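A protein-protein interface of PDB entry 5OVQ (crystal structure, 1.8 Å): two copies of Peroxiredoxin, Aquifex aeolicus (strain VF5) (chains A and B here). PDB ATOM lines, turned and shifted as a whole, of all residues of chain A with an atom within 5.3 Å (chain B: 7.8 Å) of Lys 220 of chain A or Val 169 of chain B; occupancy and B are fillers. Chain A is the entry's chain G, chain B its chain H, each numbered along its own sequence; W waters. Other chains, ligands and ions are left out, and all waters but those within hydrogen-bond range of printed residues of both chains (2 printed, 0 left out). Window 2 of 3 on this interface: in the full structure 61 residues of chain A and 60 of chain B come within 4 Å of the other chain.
The backbone NH (N) of Thr 171 of chain B lies within hydrogen-bond range of the backbone carbonyl oxygen (O) of Thr 146 of chain A.
The backbone carbonyl oxygen (O) of Ala 170 of chain B lies within hydrogen-bond range of the backbone NH (N) of Ile 192 of chain A (2.9 Å).
NE1 of Trp 175 of chain B is in hydrogen-bond range of O of Thr 189 of chain A, 2.9 Å away.
N of Val 191 of chain A lies within hydrogen-bond range of O of Lys 220 of chain A (2.8 Å).
O of Ala 164 of chain B sits at hydrogen-bond distance from N of Val 169 of chain B, at 3.4 Å.
NE of Arg 166 of chain B lies within salt-bridge range of OE2 of Glu 167 of chain B (2.9 Å).
Among the printed residues, merely in contact across the chains: Thr 146 of chain A with Ala 170 of chain B (3.3 Å), Lys 190 of chain A with Pro 172 of chain B (3.2 Å), Lys 190 of chain A with Trp 175 of chain B (3.3 Å), Val 191 of chain A with Val 169 of chain B (3.8 Å), Val 191 of chain A with Ala 170 of chain B (3.6 Å), Val 191 of chain A with Trp 175 of chain B (3.4 Å), Ile 192 of chain A with Val 169 of chain B (3.4 Å), Ile 192 of chain A with Pro 172 of chain B (3.5 Å), Pro 194 of chain A with Gly 168 of chain B (3.4 Å), Lys 220 of chain A with Val 169 of chain B (3.9 Å) and Val 222 of chain A with Glu 167 of chain B (3.3 Å).
Of the printed residues of chain B, Thr 189 of chain A touches Trp 175 (2.9 Å).
Lys 220 of chain A touches just one residue of chain B: Val 169.
Leu 161 of chain B touches none of the printed residues of chain A.
Printed residues of chain A within 4 Å of Glu 167 of chain B: Val 222 (3.3 Å).
Of chain A, only Val 191, Ile 192 and Lys 220 come within 4 Å of Val 169 of chain B.
The nearest residue of chain A that does not touch Val 169 of chain B is Pro 194 of chain A (4.1 Å).
The nearest printed residue of chain B that does not touch Val 222 of chain A is Arg 166 of chain B (4.3 Å).
Of the 13 printed residues of chain A, 8 touch a printed residue of chain B.
Hydrophobic or aromatic side chains of chain A within 4 Å of the printed part of chain B: Val 191, Ile 192, Pro 194 and Val 222.
Of the 14 printed residues of chain B, 7 touch a printed residue of chain A.
Printed residues of chain B that touch a printed residue of chain A: Glu 167, Gly 168, Val 169, Ala 170, Thr 171, Pro 172 and Trp 175.
Among the printed residues, 14 pairs touch across the chains.
No position is printed for both chains.
Of the 14 pairs that touch across the chains among the printed residues, none has its exchanged pair printed and touching as well.
Water W2 lies within hydrogen-bond range of O of Ala 160 of chain B (2.7 Å), OG1 of Thr 171 of chain B (2.8 Å) and O of Thr 146 of chain A (3.2 Å).
Water W1 bridges NZ of Lys 220 of chain A (2.8 Å) and O of Glu 167 of chain B (2.9 Å).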
ATOM      1  N   THR A 146       6.338   9.924 -12.619  1.00  0.00           N
ATOM      2  CA  THR A 146       7.632   9.324 -12.940  1.00  0.00           C
ATOM      3  C   THR A 146       7.546   7.859 -13.348  1.00  0.00           C
ATOM      4  O   THR A 146       8.503   7.344 -13.937  1.00  0.00           O
ATOM      5  CB  THR A 146       8.580   9.441 -11.747  1.00  0.00           C
ATOM      6  OG1 THR A 146       7.924   8.933 -10.576  1.00  0.00           O
ATOM      7  CG2 THR A 146       8.987  10.890 -11.517  1.00  0.00           C
ATOM      8  N   THR A 189      15.133  -2.699 -18.655  1.00  0.00           N
ATOM      9  CA  THR A 189      15.924  -1.947 -17.694  1.00  0.00           C
ATOM     10  C   THR A 189      16.218  -0.523 -18.134  1.00  0.00           C
ATOM     11  O   THR A 189      16.643   0.290 -17.305  1.00  0.00           O
ATOM     12  CB  THR A 189      17.235  -2.676 -17.395  1.00  0.00           C
ATOM     13  OG1 THR A 189      18.090  -2.643 -18.544  1.00  0.00           O
ATOM     14  CG2 THR A 189      16.937  -4.109 -17.017  1.00  0.00           C
ATOM     15  N   LYS A 190      15.947  -0.187 -19.385  1.00  0.00           N
ATOM     16  CA  LYS A 190      16.219   1.161 -19.861  1.00  0.00           C
ATOM     17  C   LYS A 190      15.290   2.148 -19.178  1.00  0.00           C
ATOM     18  O   LYS A 190      14.089   1.895 -19.052  1.00  0.00           O
ATOM     19  CB  LYS A 190      16.042   1.240 -21.377  1.00  0.00           C
ATOM     20  CG  LYS A 190      17.055   0.369 -22.139  1.00  0.00           C
ATOM     21  CD  LYS A 190      16.821   0.420 -23.622  1.00  0.00           C
ATOM     22  CE  LYS A 190      17.789  -0.504 -24.360  1.00  0.00           C
ATOM     23  NZ  LYS A 190      17.487  -0.493 -25.814  1.00  0.00           N
ATOM     24  N   VAL A 191      15.852   3.261 -18.726  1.00  0.00           N
ATOM     25  CA  VAL A 191      15.071   4.324 -18.127  1.00  0.00           C
ATOM     26  C   VAL A 191      14.804   5.405 -19.167  1.00  0.00           C
ATOM     27  O   VAL A 191      15.336   5.384 -20.275  1.00  0.00           O
ATOM     28  CB  VAL A 191      15.750   4.913 -16.877  1.00  0.00           C
ATOM     29  CG1 VAL A 191      15.853   3.853 -15.788  1.00  0.00           C
ATOM     30  CG2 VAL A 191      17.117   5.472 -17.221  1.00  0.00           C
ATOM     31  N   ILE A 192      13.954   6.357 -18.801  1.00  0.00           N
ATOM     32  CA  ILE A 192      13.451   7.394 -19.691  1.00  0.00           C
ATOM     33  C   ILE A 192      13.988   8.745 -19.234  1.00  0.00           C
ATOM     34  O   ILE A 192      13.932   9.071 -18.044  1.00  0.00           O
ATOM     35  CB  ILE A 192      11.918   7.376 -19.708  1.00  0.00           C
ATOM     36  CG1 ILE A 192      11.447   6.247 -20.625  1.00  0.00           C
ATOM     37  CG2 ILE A 192      11.369   8.739 -20.161  1.00  0.00           C
ATOM     38  CD1 ILE A 192       9.999   5.911 -20.483  1.00  0.00           C
ATOM     39  N   VAL A 193      14.512   9.521 -20.173  1.00  0.00           N
ATOM     40  CA  VAL A 193      14.917  10.901 -19.903  1.00  0.00           C
ATOM     41  C   VAL A 193      13.660  11.764 -19.831  1.00  0.00           C
ATOM     42  O   VAL A 193      12.811  11.666 -20.724  1.00  0.00           O
ATOM     43  CB  VAL A 193      15.860  11.396 -20.998  1.00  0.00           C
ATOM     44  CG1 VAL A 193      16.376  12.802 -20.692  1.00  0.00           C
ATOM     45  CG2 VAL A 193      17.009  10.403 -21.176  1.00  0.00           C
ATOM     46  N   PRO A 194      13.470  12.558 -18.782  1.00  0.00           N
ATOM     47  CA  PRO A 194      12.273  13.402 -18.711  1.00  0.00           C
ATOM     48  C   PRO A 194      12.170  14.258 -19.960  1.00  0.00           C
ATOM     49  O   PRO A 194      13.189  14.788 -20.424  1.00  0.00           O
ATOM     50  CB  PRO A 194      12.509  14.244 -17.443  1.00  0.00           C
ATOM     51  CG  PRO A 194      13.345  13.344 -16.560  1.00  0.00           C
ATOM     52  CD  PRO A 194      14.294  12.656 -17.565  1.00  0.00           C
ATOM     53  N   TYR A 210      21.188   9.941 -26.522  1.00  0.00           N
ATOM     54  CA  TYR A 210      20.281   8.916 -26.046  1.00  0.00           C
ATOM     55  C   TYR A 210      19.763   8.080 -27.217  1.00  0.00           C
ATOM     56  O   TYR A 210      19.946   8.412 -28.392  1.00  0.00           O
ATOM     57  CB  TYR A 210      19.110   9.551 -25.297  1.00  0.00           C
ATOM     58  CG  TYR A 210      19.538  10.449 -24.173  1.00  0.00           C
ATOM     59  CD1 TYR A 210      20.219   9.947 -23.062  1.00  0.00           C
ATOM     60  CD2 TYR A 210      19.240  11.808 -24.209  1.00  0.00           C
ATOM     61  CE1 TYR A 210      20.604  10.787 -22.028  1.00  0.00           C
ATOM     62  CE2 TYR A 210      19.616  12.648 -23.186  1.00  0.00           C
ATOM     63  CZ  TYR A 210      20.290  12.138 -22.094  1.00  0.00           C
ATOM     64  OH  TYR A 210      20.663  12.983 -21.069  1.00  0.00           O
ATOM     65  N   CYS A 218      13.259   9.354 -25.185  1.00  0.00           N
ATOM     66  CA  CYS A 218      14.665   8.996 -25.209  1.00  0.00           C
ATOM     67  C   CYS A 218      14.963   8.078 -24.028  1.00  0.00           C
ATOM     68  O   CYS A 218      14.532   8.354 -22.902  1.00  0.00           O
ATOM     69  CB  CYS A 218      15.539  10.243 -25.138  1.00  0.00           C
ATOM     70  SG  CYS A 218      15.349  11.334 -26.550  1.00  0.00           S
ATOM     71  N   LYS A 219      15.697   7.002 -24.290  1.00  0.00           N
ATOM     72  CA  LYS A 219      16.039   6.012 -23.281  1.00  0.00           C
ATOM     73  C   LYS A 219      17.546   5.948 -23.080  1.00  0.00           C
ATOM     74  O   LYS A 219      18.332   6.319 -23.957  1.00  0.00           O
ATOM     75  CB  LYS A 219      15.520   4.622 -23.665  1.00  0.00           C
ATOM     76  CG  LYS A 219      14.013   4.501 -23.677  1.00  0.00           C
ATOM     77  CD  LYS A 219      13.565   3.181 -24.283  1.00  0.00           C
ATOM     78  CE  LYS A 219      12.047   3.088 -24.292  1.00  0.00           C
ATOM     79  NZ  LYS A 219      11.549   1.922 -25.068  1.00  0.00           N
ATOM     80  N   LYS A 220      17.938   5.467 -21.903  1.00  0.00           N
ATOM     81  CA  LYS A 220      19.326   5.154 -21.603  1.00  0.00           C
ATOM     82  C   LYS A 220      19.332   4.077 -20.531  1.00  0.00           C
ATOM     83  O   LYS A 220      18.285   3.664 -20.032  1.00  0.00           O
ATOM     84  CB  LYS A 220      20.107   6.388 -21.140  1.00  0.00           C
ATOM     85  CG  LYS A 220      19.561   7.000 -19.856  1.00  0.00           C
ATOM     86  CD  LYS A 220      20.445   8.125 -19.362  1.00  0.00           C
ATOM     87  CE  LYS A 220      20.040   8.566 -17.971  1.00  0.00           C
ATOM     88  NZ  LYS A 220      20.911   9.659 -17.466  1.00  0.00           N
ATOM     89  N   LYS A 221      20.515   3.611 -20.183  1.00  0.00           N
ATOM     90  CA  LYS A 221      20.637   2.724 -19.042  1.00  0.00           C
ATOM     91  C   LYS A 221      21.336   3.476 -17.923  1.00  0.00           C
ATOM     92  O   LYS A 221      22.079   4.431 -18.168  1.00  0.00           O
ATOM     93  CB  LYS A 221      21.391   1.449 -19.425  1.00  0.00           C
ATOM     94  CG  LYS A 221      20.576   0.574 -20.363  1.00  0.00           C
ATOM     95  CD  LYS A 221      21.280  -0.716 -20.724  1.00  0.00           C
ATOM     96  CE  LYS A 221      20.454  -1.499 -21.731  1.00  0.00           C
ATOM     97  NZ  LYS A 221      21.143  -2.741 -22.148  1.00  0.00           N
ATOM     98  N   VAL A 222      21.068   3.060 -16.690  1.00  0.00           N
ATOM     99  CA  VAL A 222      21.713   3.671 -15.541  1.00  0.00           C
ATOM    100  C   VAL A 222      22.795   2.738 -15.017  1.00  0.00           C
ATOM    101  O   VAL A 222      22.553   1.544 -14.855  1.00  0.00           O
ATOM    102  CB  VAL A 222      20.694   4.005 -14.446  1.00  0.00           C
ATOM    103  CG1 VAL A 222      21.405   4.212 -13.128  1.00  0.00           C
ATOM    104  CG2 VAL A 222      19.899   5.243 -14.831  1.00  0.00           C
ATOM    105  N   ALA B 160      11.539   1.537  -8.727  1.00  0.00           N
ATOM    106  CA  ALA B 160      11.276   2.550  -9.748  1.00  0.00           C
ATOM    107  C   ALA B 160      11.292   3.957  -9.160  1.00  0.00           C
ATOM    108  O   ALA B 160      11.855   4.878  -9.754  1.00  0.00           O
ATOM    109  CB  ALA B 160       9.937   2.262 -10.418  1.00  0.00           C
ATOM    110  N   LEU B 161      10.692   4.141  -7.983  1.00  0.00           N
ATOM    111  CA  LEU B 161      10.690   5.465  -7.375  1.00  0.00           C
ATOM    112  C   LEU B 161      12.086   5.861  -6.904  1.00  0.00           C
ATOM    113  O   LEU B 161      12.496   7.014  -7.069  1.00  0.00           O
ATOM    114  CB  LEU B 161       9.689   5.505  -6.211  1.00  0.00           C
ATOM    115  CG  LEU B 161       8.226   5.411  -6.642  1.00  0.00           C
ATOM    116  CD1 LEU B 161       7.356   4.980  -5.466  1.00  0.00           C
ATOM    117  CD2 LEU B 161       7.752   6.762  -7.170  1.00  0.00           C
ATOM    118  N   GLN B 162      12.829   4.928  -6.305  1.00  0.00           N
ATOM    119  CA  GLN B 162      14.160   5.285  -5.825  1.00  0.00           C
ATOM    120  C   GLN B 162      15.099   5.585  -6.985  1.00  0.00           C
ATOM    121  O   GLN B 162      15.902   6.525  -6.914  1.00  0.00           O
ATOM    122  CB  GLN B 162      14.713   4.180  -4.928  1.00  0.00           C
ATOM    123  CG  GLN B 162      13.934   4.068  -3.614  1.00  0.00           C
ATOM    124  CD  GLN B 162      14.496   3.017  -2.686  1.00  0.00           C
ATOM    125  OE1 GLN B 162      15.227   2.115  -3.117  1.00  0.00           O
ATOM    126  NE2 GLN B 162      14.150   3.110  -1.402  1.00  0.00           N
ATOM    127  N   THR B 163      14.981   4.829  -8.078  1.00  0.00           N
ATOM    128  CA  THR B 163      15.790   5.108  -9.259  1.00  0.00           C
ATOM    129  C   THR B 163      15.439   6.463  -9.856  1.00  0.00           C
ATOM    130  O   THR B 163      16.328   7.227 -10.254  1.00  0.00           O
ATOM    131  CB  THR B 163      15.590   4.009 -10.303  1.00  0.00           C
ATOM    132  OG1 THR B 163      16.100   2.777  -9.791  1.00  0.00           O
ATOM    133  CG2 THR B 163      16.322   4.358 -11.607  1.00  0.00           C
ATOM    134  N   ALA B 164      14.143   6.767  -9.943  1.00  0.00           N
ATOM    135  CA  ALA B 164      13.713   8.069 -10.446  1.00  0.00           C
ATOM    136  C   ALA B 164      14.325   9.197  -9.620  1.00  0.00           C
ATOM    137  O   ALA B 164      14.872  10.158 -10.171  1.00  0.00           O
ATOM    138  CB  ALA B 164      12.185   8.147 -10.449  1.00  0.00           C
ATOM    139  N   ASP B 165      14.261   9.084  -8.288  1.00  0.00           N
ATOM    140  CA  ASP B 165      14.827  10.116  -7.418  1.00  0.00           C
ATOM    141  C   ASP B 165      16.344  10.196  -7.545  1.00  0.00           C
ATOM    142  O   ASP B 165      16.912  11.295  -7.614  1.00  0.00           O
ATOM    143  CB  ASP B 165      14.441   9.853  -5.966  1.00  0.00           C
ATOM    144  CG  ASP B 165      12.978  10.133  -5.690  1.00  0.00           C
ATOM    145  OD1 ASP B 165      12.262  10.569  -6.616  1.00  0.00           O
ATOM    146  OD2 ASP B 165      12.553   9.912  -4.535  1.00  0.00           O
ATOM    147  N   ARG B 166      17.016   9.049  -7.553  1.00  0.00           N
ATOM    148  CA  ARG B 166      18.476   9.035  -7.556  1.00  0.00           C
ATOM    149  C   ARG B 166      19.044   9.543  -8.875  1.00  0.00           C
ATOM    150  O   ARG B 166      20.000  10.325  -8.888  1.00  0.00           O
ATOM    151  CB  ARG B 166      18.977   7.618  -7.291  1.00  0.00           C
ATOM    152  CG  ARG B 166      20.493   7.494  -7.207  1.00  0.00           C
ATOM    153  CD  ARG B 166      20.935   6.036  -7.096  1.00  0.00           C
ATOM    154  NE  ARG B 166      20.572   5.253  -8.277  1.00  0.00           N
ATOM    155  CZ  ARG B 166      19.601   4.346  -8.306  1.00  0.00           C
ATOM    156  NH1 ARG B 166      18.894   4.100  -7.208  1.00  0.00           N
ATOM    157  NH2 ARG B 166      19.343   3.679  -9.426  1.00  0.00           N
ATOM    158  N   GLU B 167      18.463   9.122  -9.993  1.00  0.00           N
ATOM    159  CA  GLU B 167      19.036   9.394 -11.304  1.00  0.00           C
ATOM    160  C   GLU B 167      18.361  10.535 -12.052  1.00  0.00           C
ATOM    161  O   GLU B 167      18.850  10.918 -13.120  1.00  0.00           O
ATOM    162  CB  GLU B 167      19.004   8.130 -12.169  1.00  0.00           C
ATOM    163  CG  GLU B 167      19.678   6.931 -11.516  1.00  0.00           C
ATOM    164  CD  GLU B 167      21.184   7.087 -11.435  1.00  0.00           C
ATOM    165  OE1 GLU B 167      21.745   7.876 -12.225  1.00  0.00           O
ATOM    166  OE2 GLU B 167      21.809   6.424 -10.583  1.00  0.00           O
ATOM    167  N   GLY B 168      17.259  11.078 -11.543  1.00  0.00           N
ATOM    168  CA  GLY B 168      16.552  12.106 -12.292  1.00  0.00           C
ATOM    169  C   GLY B 168      15.957  11.594 -13.588  1.00  0.00           C
ATOM    170  O   GLY B 168      16.045  12.269 -14.625  1.00  0.00           O
ATOM    171  N   VAL B 169      15.344  10.417 -13.553  1.00  0.00           N
ATOM    172  CA  VAL B 169      14.784   9.781 -14.731  1.00  0.00           C
ATOM    173  C   VAL B 169      13.350   9.390 -14.419  1.00  0.00           C
ATOM    174  O   VAL B 169      12.873   9.514 -13.288  1.00  0.00           O
ATOM    175  CB  VAL B 169      15.598   8.540 -15.178  1.00  0.00           C
ATOM    176  CG1 VAL B 169      17.005   8.933 -15.575  1.00  0.00           C
ATOM    177  CG2 VAL B 169      15.656   7.480 -14.055  1.00  0.00           C
ATOM    178  N   ALA B 170      12.655   8.946 -15.452  1.00  0.00           N
ATOM    179  CA  ALA B 170      11.379   8.271 -15.301  1.00  0.00           C
ATOM    180  C   ALA B 170      11.564   6.808 -15.669  1.00  0.00           C
ATOM    181  O   ALA B 170      12.575   6.425 -16.267  1.00  0.00           O
ATOM    182  CB  ALA B 170      10.300   8.928 -16.176  1.00  0.00           C
ATOM    183  N   THR B 171      10.604   5.978 -15.268  1.00  0.00           N
ATOM    184  CA  THR B 171      10.754   4.579 -15.625  1.00  0.00           C
ATOM    185  C   THR B 171       9.593   4.146 -16.508  1.00  0.00           C
ATOM    186  O   THR B 171       8.447   4.539 -16.269  1.00  0.00           O
ATOM    187  CB  THR B 171      10.852   3.648 -14.393  1.00  0.00           C
ATOM    188  OG1 THR B 171       9.693   3.799 -13.567  1.00  0.00           O
ATOM    189  CG2 THR B 171      12.092   3.988 -13.592  1.00  0.00           C
ATOM    190  N   PRO B 172       9.873   3.398 -17.568  1.00  0.00           N
ATOM    191  CA  PRO B 172       8.822   3.016 -18.512  1.00  0.00           C
ATOM    192  C   PRO B 172       7.928   1.932 -17.944  1.00  0.00           C
ATOM    193  O   PRO B 172       8.179   1.363 -16.878  1.00  0.00           O
ATOM    194  CB  PRO B 172       9.617   2.499 -19.716  1.00  0.00           C
ATOM    195  CG  PRO B 172      10.865   1.974 -19.107  1.00  0.00           C
ATOM    196  CD  PRO B 172      11.198   2.912 -17.987  1.00  0.00           C
ATOM    197  N   TRP B 175       9.221  -1.574 -16.157  1.00  0.00           N
ATOM    198  CA  TRP B 175      10.632  -1.351 -15.883  1.00  0.00           C
ATOM    199  C   TRP B 175      11.109  -2.172 -14.697  1.00  0.00           C
ATOM    200  O   TRP B 175      10.419  -2.276 -13.684  1.00  0.00           O
ATOM    201  CB  TRP B 175      10.892   0.117 -15.576  1.00  0.00           C
ATOM    202  CG  TRP B 175      12.316   0.380 -15.232  1.00  0.00           C
ATOM    203  CD1 TRP B 175      13.336   0.610 -16.108  1.00  0.00           C
ATOM    204  CD2 TRP B 175      12.893   0.417 -13.923  1.00  0.00           C
ATOM    205  NE1 TRP B 175      14.514   0.799 -15.424  1.00  0.00           N
ATOM    206  CE2 TRP B 175      14.265   0.689 -14.079  1.00  0.00           C
ATOM    207  CE3 TRP B 175      12.381   0.250 -12.630  1.00  0.00           C
ATOM    208  CZ2 TRP B 175      15.129   0.803 -12.995  1.00  0.00           C
ATOM    209  CZ3 TRP B 175      13.240   0.368 -11.558  1.00  0.00           C
ATOM    210  CH2 TRP B 175      14.599   0.640 -11.745  1.00  0.00           C
HETATM  211  O   HOH W   1      20.963   9.780 -14.717  1.00  0.00           O
HETATM  212  O   HOH W   2       9.950   5.746 -11.512  1.00  0.00           O
